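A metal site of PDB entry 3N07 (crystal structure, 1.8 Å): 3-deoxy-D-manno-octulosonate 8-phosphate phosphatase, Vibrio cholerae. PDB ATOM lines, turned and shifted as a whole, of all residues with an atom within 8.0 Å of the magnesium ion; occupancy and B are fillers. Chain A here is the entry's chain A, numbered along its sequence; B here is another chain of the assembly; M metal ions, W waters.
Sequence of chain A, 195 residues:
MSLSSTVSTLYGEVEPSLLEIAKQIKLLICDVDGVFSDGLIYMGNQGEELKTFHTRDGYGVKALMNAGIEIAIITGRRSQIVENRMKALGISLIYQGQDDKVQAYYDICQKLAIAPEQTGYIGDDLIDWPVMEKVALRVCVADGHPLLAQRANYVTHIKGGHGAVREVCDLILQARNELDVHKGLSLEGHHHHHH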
ATOM      1  N   CYS A  30     -32.174 -19.916   7.639  1.00  0.00           N
ATOM      2  CA  CYS A  30     -32.012 -18.763   8.538  1.00  0.00           C
ATOM      3  C   CYS A  30     -30.647 -18.124   8.372  1.00  0.00           C
ATOM      4  O   CYS A  30     -29.638 -18.824   8.238  1.00  0.00           O
ATOM      5  CB  CYS A  30     -32.117 -19.209   9.985  1.00  0.00           C
ATOM      6  SG  CYS A  30     -33.733 -19.966  10.383  1.00  0.00           S
ATOM      7  N   ASP A  31     -30.638 -16.803   8.363  1.00  0.00           N
ATOM      8  CA  ASP A  31     -29.460 -16.035   8.719  1.00  0.00           C
ATOM      9  C   ASP A  31     -29.135 -16.236  10.211  1.00  0.00           C
ATOM     10  O   ASP A  31     -29.989 -16.702  11.004  1.00  0.00           O
ATOM     11  CB  ASP A  31     -29.723 -14.548   8.415  1.00  0.00           C
ATOM     12  CG  ASP A  31     -28.527 -13.682   8.729  1.00  0.00           C
ATOM     13  OD1 ASP A  31     -27.403 -14.030   8.297  1.00  0.00           O
ATOM     14  OD2 ASP A  31     -28.717 -12.660   9.434  1.00  0.00           O
ATOM     15  N   VAL A  32     -27.909 -15.909  10.636  1.00  0.00           N
ATOM     16  CA  VAL A  32     -27.542 -16.012  12.062  1.00  0.00           C
ATOM     17  C   VAL A  32     -27.574 -14.665  12.771  1.00  0.00           C
ATOM     18  O   VAL A  32     -28.384 -14.447  13.682  1.00  0.00           O
ATOM     19  CB  VAL A  32     -26.142 -16.696  12.314  1.00  0.00           C
ATOM     20  CG1 VAL A  32     -25.855 -16.732  13.828  1.00  0.00           C
ATOM     21  CG2 VAL A  32     -26.154 -18.111  11.802  1.00  0.00           C
ATOM     22  N   ASP A  33     -26.695 -13.758  12.376  1.00  0.00           N
ATOM     23  CA  ASP A  33     -26.538 -12.510  13.143  1.00  0.00           C
ATOM     24  C   ASP A  33     -27.723 -11.586  12.938  1.00  0.00           C
ATOM     25  O   ASP A  33     -28.046 -11.212  11.811  1.00  0.00           O
ATOM     26  CB  ASP A  33     -25.247 -11.797  12.713  1.00  0.00           C
ATOM     27  CG  ASP A  33     -24.010 -12.627  13.023  1.00  0.00           C
ATOM     28  OD1 ASP A  33     -23.689 -12.767  14.208  1.00  0.00           O
ATOM     29  OD2 ASP A  33     -23.371 -13.090  12.049  1.00  0.00           O
ATOM     30  N   GLY A  34     -28.395 -11.258  14.027  1.00  0.00           N
ATOM     31  CA  GLY A  34     -29.591 -10.433  13.944  1.00  0.00           C
ATOM     32  C   GLY A  34     -30.881 -11.252  13.874  1.00  0.00           C
ATOM     33  O   GLY A  34     -31.976 -10.686  13.945  1.00  0.00           O
ATOM     34  N   VAL A  35     -30.746 -12.580  13.749  1.00  0.00           N
ATOM     35  CA  VAL A  35     -31.904 -13.505  13.668  1.00  0.00           C
ATOM     36  C   VAL A  35     -31.844 -14.503  14.851  1.00  0.00           C
ATOM     37  O   VAL A  35     -32.682 -14.452  15.758  1.00  0.00           O
ATOM     38  CB  VAL A  35     -31.942 -14.202  12.306  1.00  0.00           C
ATOM     39  CG1 VAL A  35     -32.968 -15.387  12.313  1.00  0.00           C
ATOM     40  CG2 VAL A  35     -32.202 -13.162  11.188  1.00  0.00           C
ATOM     41  N   PHE A  36     -30.864 -15.393  14.850  1.00  0.00           N
ATOM     42  CA  PHE A  36     -30.581 -16.224  16.027  1.00  0.00           C
ATOM     43  C   PHE A  36     -29.912 -15.415  17.151  1.00  0.00           C
ATOM     44  O   PHE A  36     -30.143 -15.684  18.320  1.00  0.00           O
ATOM     45  CB  PHE A  36     -29.678 -17.391  15.633  1.00  0.00           C
ATOM     46  CG  PHE A  36     -30.440 -18.620  15.131  1.00  0.00           C
ATOM     47  CD1 PHE A  36     -30.907 -19.561  16.062  1.00  0.00           C
ATOM     48  CD2 PHE A  36     -30.626 -18.855  13.778  1.00  0.00           C
ATOM     49  CE1 PHE A  36     -31.589 -20.695  15.653  1.00  0.00           C
ATOM     50  CE2 PHE A  36     -31.306 -19.995  13.346  1.00  0.00           C
ATOM     51  CZ  PHE A  36     -31.768 -20.925  14.282  1.00  0.00           C
ATOM     52  N   SER A  37     -29.145 -14.379  16.783  1.00  0.00           N
ATOM     53  CA  SER A  37     -28.484 -13.513  17.798  1.00  0.00           C
ATOM     54  C   SER A  37     -29.137 -12.148  17.803  1.00  0.00           C
ATOM     55  O   SER A  37     -29.926 -11.824  16.920  1.00  0.00           O
ATOM     56  CB  SER A  37     -27.005 -13.362  17.467  1.00  0.00           C
ATOM     57  OG  SER A  37     -26.872 -12.413  16.426  1.00  0.00           O
ATOM     58  N   GLY A  39     -27.717  -9.511  16.908  1.00  0.00           N
ATOM     59  CA  GLY A  39     -26.929  -8.704  15.988  1.00  0.00           C
ATOM     60  C   GLY A  39     -25.594  -8.192  16.522  1.00  0.00           C
ATOM     61  O   GLY A  39     -24.832  -7.553  15.789  1.00  0.00           O
ATOM     62  N   ILE A  74     -27.386 -19.824   6.537  1.00  0.00           N
ATOM     63  CA  ILE A  74     -26.453 -19.115   5.648  1.00  0.00           C
ATOM     64  C   ILE A  74     -26.057 -17.802   6.285  1.00  0.00           C
ATOM     65  O   ILE A  74     -26.910 -16.925   6.479  1.00  0.00           O
ATOM     66  CB  ILE A  74     -27.052 -18.812   4.231  1.00  0.00           C
ATOM     67  CG1 ILE A  74     -27.760 -20.028   3.631  1.00  0.00           C
ATOM     68  CG2 ILE A  74     -25.916 -18.304   3.275  1.00  0.00           C
ATOM     69  CD1 ILE A  74     -28.465 -19.741   2.302  1.00  0.00           C
ATOM     70  N   THR A  75     -24.763 -17.668   6.590  1.00  0.00           N
ATOM     71  CA  THR A  75     -24.247 -16.507   7.287  1.00  0.00           C
ATOM     72  C   THR A  75     -23.002 -15.980   6.547  1.00  0.00           C
ATOM     73  O   THR A  75     -22.308 -16.740   5.866  1.00  0.00           O
ATOM     74  CB  THR A  75     -23.995 -16.831   8.803  1.00  0.00           C
ATOM     75  OG1 THR A  75     -23.480 -15.666   9.477  1.00  0.00           O
ATOM     76  CG2 THR A  75     -23.013 -17.991   8.957  1.00  0.00           C
ATOM     77  N   GLY A  76     -22.764 -14.677   6.637  1.00  0.00           N
ATOM     78  CA  GLY A  76     -21.627 -14.044   5.953  1.00  0.00           C
ATOM     79  C   GLY A  76     -20.391 -14.077   6.823  1.00  0.00           C
ATOM     80  O   GLY A  76     -19.262 -13.965   6.317  1.00  0.00           O
ATOM     81  N   LYS A 101     -25.156 -14.954  -0.763  1.00  0.00           N
ATOM     82  CA  LYS A 101     -25.964 -16.022  -0.220  1.00  0.00           C
ATOM     83  C   LYS A 101     -26.725 -16.830  -1.269  1.00  0.00           C
ATOM     84  O   LYS A 101     -27.205 -17.933  -0.972  1.00  0.00           O
ATOM     85  CB  LYS A 101     -26.907 -15.442   0.812  1.00  0.00           C
ATOM     86  CG  LYS A 101     -26.165 -14.817   1.968  1.00  0.00           C
ATOM     87  CD  LYS A 101     -27.061 -14.645   3.177  1.00  0.00           C
ATOM     88  CE  LYS A 101     -26.243 -14.107   4.360  1.00  0.00           C
ATOM     89  NZ  LYS A 101     -27.015 -14.173   5.639  1.00  0.00           N
ATOM     90  N   TYR A 121     -37.450 -18.290   4.545  1.00  0.00           N
ATOM     91  CA  TYR A 121     -36.182 -17.701   4.941  1.00  0.00           C
ATOM     92  C   TYR A 121     -36.388 -16.602   5.976  1.00  0.00           C
ATOM     93  O   TYR A 121     -37.214 -15.725   5.778  1.00  0.00           O
ATOM     94  CB  TYR A 121     -35.480 -17.104   3.712  1.00  0.00           C
ATOM     95  CG  TYR A 121     -34.067 -16.643   3.939  1.00  0.00           C
ATOM     96  CD1 TYR A 121     -33.779 -15.509   4.748  1.00  0.00           C
ATOM     97  CD2 TYR A 121     -33.006 -17.282   3.284  1.00  0.00           C
ATOM     98  CE1 TYR A 121     -32.442 -15.076   4.935  1.00  0.00           C
ATOM     99  CE2 TYR A 121     -31.697 -16.867   3.466  1.00  0.00           C
ATOM    100  CZ  TYR A 121     -31.416 -15.769   4.284  1.00  0.00           C
ATOM    101  OH  TYR A 121     -30.101 -15.376   4.417  1.00  0.00           O
ATOM    102  N   ILE A 122     -35.594 -16.617   7.053  1.00  0.00           N
ATOM    103  CA  ILE A 122     -35.639 -15.569   8.060  1.00  0.00           C
ATOM    104  C   ILE A 122     -34.355 -14.715   7.981  1.00  0.00           C
ATOM    105  O   ILE A 122     -33.255 -15.209   8.246  1.00  0.00           O
ATOM    106  CB  ILE A 122     -35.764 -16.128   9.510  1.00  0.00           C
ATOM    107  CG1 ILE A 122     -36.891 -17.165   9.587  1.00  0.00           C
ATOM    108  CG2 ILE A 122     -35.932 -14.960  10.525  1.00  0.00           C
ATOM    109  CD1 ILE A 122     -36.935 -17.897  10.953  1.00  0.00           C
ATOM    110  N   GLY A 123     -34.506 -13.434   7.661  1.00  0.00           N
ATOM    111  CA  GLY A 123     -33.355 -12.530   7.599  1.00  0.00           C
ATOM    112  C   GLY A 123     -33.507 -11.255   8.384  1.00  0.00           C
ATOM    113  O   GLY A 123     -34.572 -11.016   9.008  1.00  0.00           O
ATOM    114  N   ASP A 124     -32.448 -10.422   8.386  1.00  0.00           N
ATOM    115  CA  ASP A 124     -32.522  -9.137   9.072  1.00  0.00           C
ATOM    116  C   ASP A 124     -31.885  -7.978   8.296  1.00  0.00           C
ATOM    117  O   ASP A 124     -31.950  -6.855   8.758  1.00  0.00           O
ATOM    118  CB  ASP A 124     -31.892  -9.183  10.464  1.00  0.00           C
ATOM    119  CG  ASP A 124     -30.405  -9.182  10.406  1.00  0.00           C
ATOM    120  OD1 ASP A 124     -29.859 -10.051   9.710  1.00  0.00           O
ATOM    121  OD2 ASP A 124     -29.756  -8.296  11.030  1.00  0.00           O
ATOM    122  N   ASP A 125     -31.274  -8.250   7.143  1.00  0.00           N
ATOM    123  CA  ASP A 125     -30.597  -7.186   6.378  1.00  0.00           C
ATOM    124  C   ASP A 125     -30.662  -7.431   4.870  1.00  0.00           C
ATOM    125  O   ASP A 125     -31.132  -8.482   4.426  1.00  0.00           O
ATOM    126  CB  ASP A 125     -29.166  -6.960   6.899  1.00  0.00           C
ATOM    127  CG  ASP A 125     -28.666  -5.538   6.638  1.00  0.00           C
ATOM    128  OD1 ASP A 125     -29.354  -4.736   5.948  1.00  0.00           O
ATOM    129  OD2 ASP A 125     -27.570  -5.209   7.122  1.00  0.00           O
ATOM    130  N   LEU A 126     -30.179  -6.468   4.086  1.00  0.00           N
ATOM    131  CA  LEU A 126     -30.413  -6.458   2.641  1.00  0.00           C
ATOM    132  C   LEU A 126     -29.749  -7.613   1.909  1.00  0.00           C
ATOM    133  O   LEU A 126     -30.256  -8.065   0.866  1.00  0.00           O
ATOM    134  CB  LEU A 126     -29.968  -5.124   2.041  1.00  0.00           C
ATOM    135  CG  LEU A 126     -30.774  -3.930   2.526  1.00  0.00           C
ATOM    136  CD1 LEU A 126     -30.301  -2.711   1.780  1.00  0.00           C
ATOM    137  CD2 LEU A 126     -32.270  -4.146   2.328  1.00  0.00           C
ATOM    138  N   ILE A 127     -28.634  -8.099   2.473  1.00  0.00           N
ATOM    139  CA  ILE A 127     -27.922  -9.255   1.905  1.00  0.00           C
ATOM    140  C   ILE A 127     -28.797 -10.529   1.902  1.00  0.00           C
ATOM    141  O   ILE A 127     -28.552 -11.474   1.163  1.00  0.00           O
ATOM    142  CB  ILE A 127     -26.561  -9.513   2.647  1.00  0.00           C
ATOM    143  CG1 ILE A 127     -25.664 -10.462   1.823  1.00  0.00           C
ATOM    144  CG2 ILE A 127     -26.791 -10.000   4.043  1.00  0.00           C
ATOM    145  CD1 ILE A 127     -25.093  -9.826   0.564  1.00  0.00           C
ATOM    146  N   ASP A 128     -29.845 -10.531   2.730  1.00  0.00           N
ATOM    147  CA  ASP A 128     -30.723 -11.671   2.811  1.00  0.00           C
ATOM    148  C   ASP A 128     -31.773 -11.638   1.714  1.00  0.00           C
ATOM    149  O   ASP A 128     -32.320 -12.686   1.362  1.00  0.00           O
ATOM    150  CB  ASP A 128     -31.415 -11.715   4.173  1.00  0.00           C
ATOM    151  CG  ASP A 128     -30.421 -11.921   5.308  1.00  0.00           C
ATOM    152  OD1 ASP A 128     -29.631 -12.870   5.235  1.00  0.00           O
ATOM    153  OD2 ASP A 128     -30.438 -11.142   6.269  1.00  0.00           O
ATOM    154  N   VAL A 141     -37.091 -10.099  10.766  1.00  0.00           N
ATOM    155  CA  VAL A 141     -37.317  -9.947  12.218  1.00  0.00           C
ATOM    156  C   VAL A 141     -37.762  -8.525  12.592  1.00  0.00           C
ATOM    157  O   VAL A 141     -37.499  -7.574  11.850  1.00  0.00           O
ATOM    158  CB  VAL A 141     -36.073 -10.374  13.053  1.00  0.00           C
ATOM    159  CG1 VAL A 141     -35.704 -11.875  12.759  1.00  0.00           C
ATOM    160  CG2 VAL A 141     -34.876  -9.411  12.792  1.00  0.00           C
ATOM    161  N   LEU A 148     -35.659  -4.157   4.377  1.00  0.00           N
ATOM    162  CA  LEU A 148     -36.040  -5.584   4.316  1.00  0.00           C
ATOM    163  C   LEU A 148     -37.455  -5.802   4.854  1.00  0.00           C
ATOM    164  O   LEU A 148     -38.238  -6.558   4.281  1.00  0.00           O
ATOM    165  CB  LEU A 148     -35.076  -6.475   5.113  1.00  0.00           C
ATOM    166  CG  LEU A 148     -35.155  -7.974   4.784  1.00  0.00           C
ATOM    167  CD1 LEU A 148     -34.586  -8.257   3.365  1.00  0.00           C
ATOM    168  CD2 LEU A 148     -34.481  -8.850   5.827  1.00  0.00           C
ATOM    169  N   HIS B  54     -22.320  -3.859  16.218  1.00  0.00           N
ATOM    170  CA  HIS B  54     -23.512  -4.401  15.565  1.00  0.00           C
ATOM    171  C   HIS B  54     -23.255  -4.796  14.098  1.00  0.00           C
ATOM    172  O   HIS B  54     -22.653  -4.042  13.334  1.00  0.00           O
ATOM    173  CB  HIS B  54     -24.651  -3.402  15.634  1.00  0.00           C
ATOM    174  CG  HIS B  54     -26.003  -4.040  15.436  1.00  0.00           C
ATOM    175  ND1 HIS B  54     -26.515  -4.288  14.183  1.00  0.00           N
ATOM    176  CD2 HIS B  54     -26.922  -4.499  16.316  1.00  0.00           C
ATOM    177  CE1 HIS B  54     -27.689  -4.881  14.305  1.00  0.00           C
ATOM    178  NE2 HIS B  54     -27.961  -5.012  15.588  1.00  0.00           N
ATOM    179  N   THR B  55     -23.749  -5.971  13.719  1.00  0.00           N
ATOM    180  CA  THR B  55     -23.572  -6.449  12.341  1.00  0.00           C
ATOM    181  C   THR B  55     -24.172  -5.545  11.270  1.00  0.00           C
ATOM    182  O   THR B  55     -23.644  -5.481  10.172  1.00  0.00           O
ATOM    183  CB  THR B  55     -23.995  -7.905  12.121  1.00  0.00           C
ATOM    184  OG1 THR B  55     -25.370  -8.127  12.506  1.00  0.00           O
ATOM    185  CG2 THR B  55     -23.104  -8.819  12.915  1.00  0.00           C
ATOM    186  N   ARG B  56     -25.239  -4.827  11.565  1.00  0.00           N
ATOM    187  CA  ARG B  56     -25.831  -4.018  10.502  1.00  0.00           C
ATOM    188  C   ARG B  56     -24.977  -2.763  10.200  1.00  0.00           C
ATOM    189  O   ARG B  56     -25.077  -2.177   9.115  1.00  0.00           O
ATOM    190  CB  ARG B  56     -27.290  -3.691  10.815  1.00  0.00           C
ATOM    191  CG  ARG B  56     -28.252  -4.871  10.592  1.00  0.00           C
ATOM    192  CD  ARG B  56     -29.732  -4.427  10.606  1.00  0.00           C
ATOM    193  NE  ARG B  56     -30.221  -4.125  11.940  1.00  0.00           N
ATOM    194  CZ  ARG B  56     -30.701  -5.034  12.786  1.00  0.00           C
ATOM    195  NH1 ARG B  56     -30.772  -6.298  12.395  1.00  0.00           N
ATOM    196  NH2 ARG B  56     -31.083  -4.693  14.019  1.00  0.00           N
HETATM  197 MG    MG M   1     -27.902 -10.889   9.650  1.00  0.00          MG
HETATM  198  O   HOH W   1     -27.966 -10.576   7.479  1.00  0.00           O
HETATM  199  O   HOH W   2     -27.231  -8.704  10.297  1.00  0.00           O
HETATM  200  O   HOH W   3     -25.907 -11.409   9.351  1.00  0.00           O
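Water W2 bridges OD2 of Asp 124 (2.7 Å) and OG1 of Thr 55 of chain B (2.9 Å).
The side-chain carboxylate of Asp 31 lies within salt-bridge range of the side-chain amino group of Lys 101 (2.7 Å).
O of Ile 122 sits at hydrogen-bond distance from N of Asp 31, 3.1 Å away.
The backbone NH of Asp 124 lies within hydrogen-bond range of the side-chain carboxylate of Asp 128, at 3.0 Å.
The guanidinium group of Arg 56 of chain B lies within salt-bridge range of the side-chain carboxylate of Asp 124.
Within 4 Å of the magnesium ion: Asp 31, Asp 33 and Asp 124.
The magnesium ion is bound by OD2 of Asp 31 (2.0 Å), water W3 (2.1 Å), OD1 of Asp 124 (2.1 Å), O of Asp 33 (2.2 Å), water W1 (2.2 Å) and water W2 (2.4 Å).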
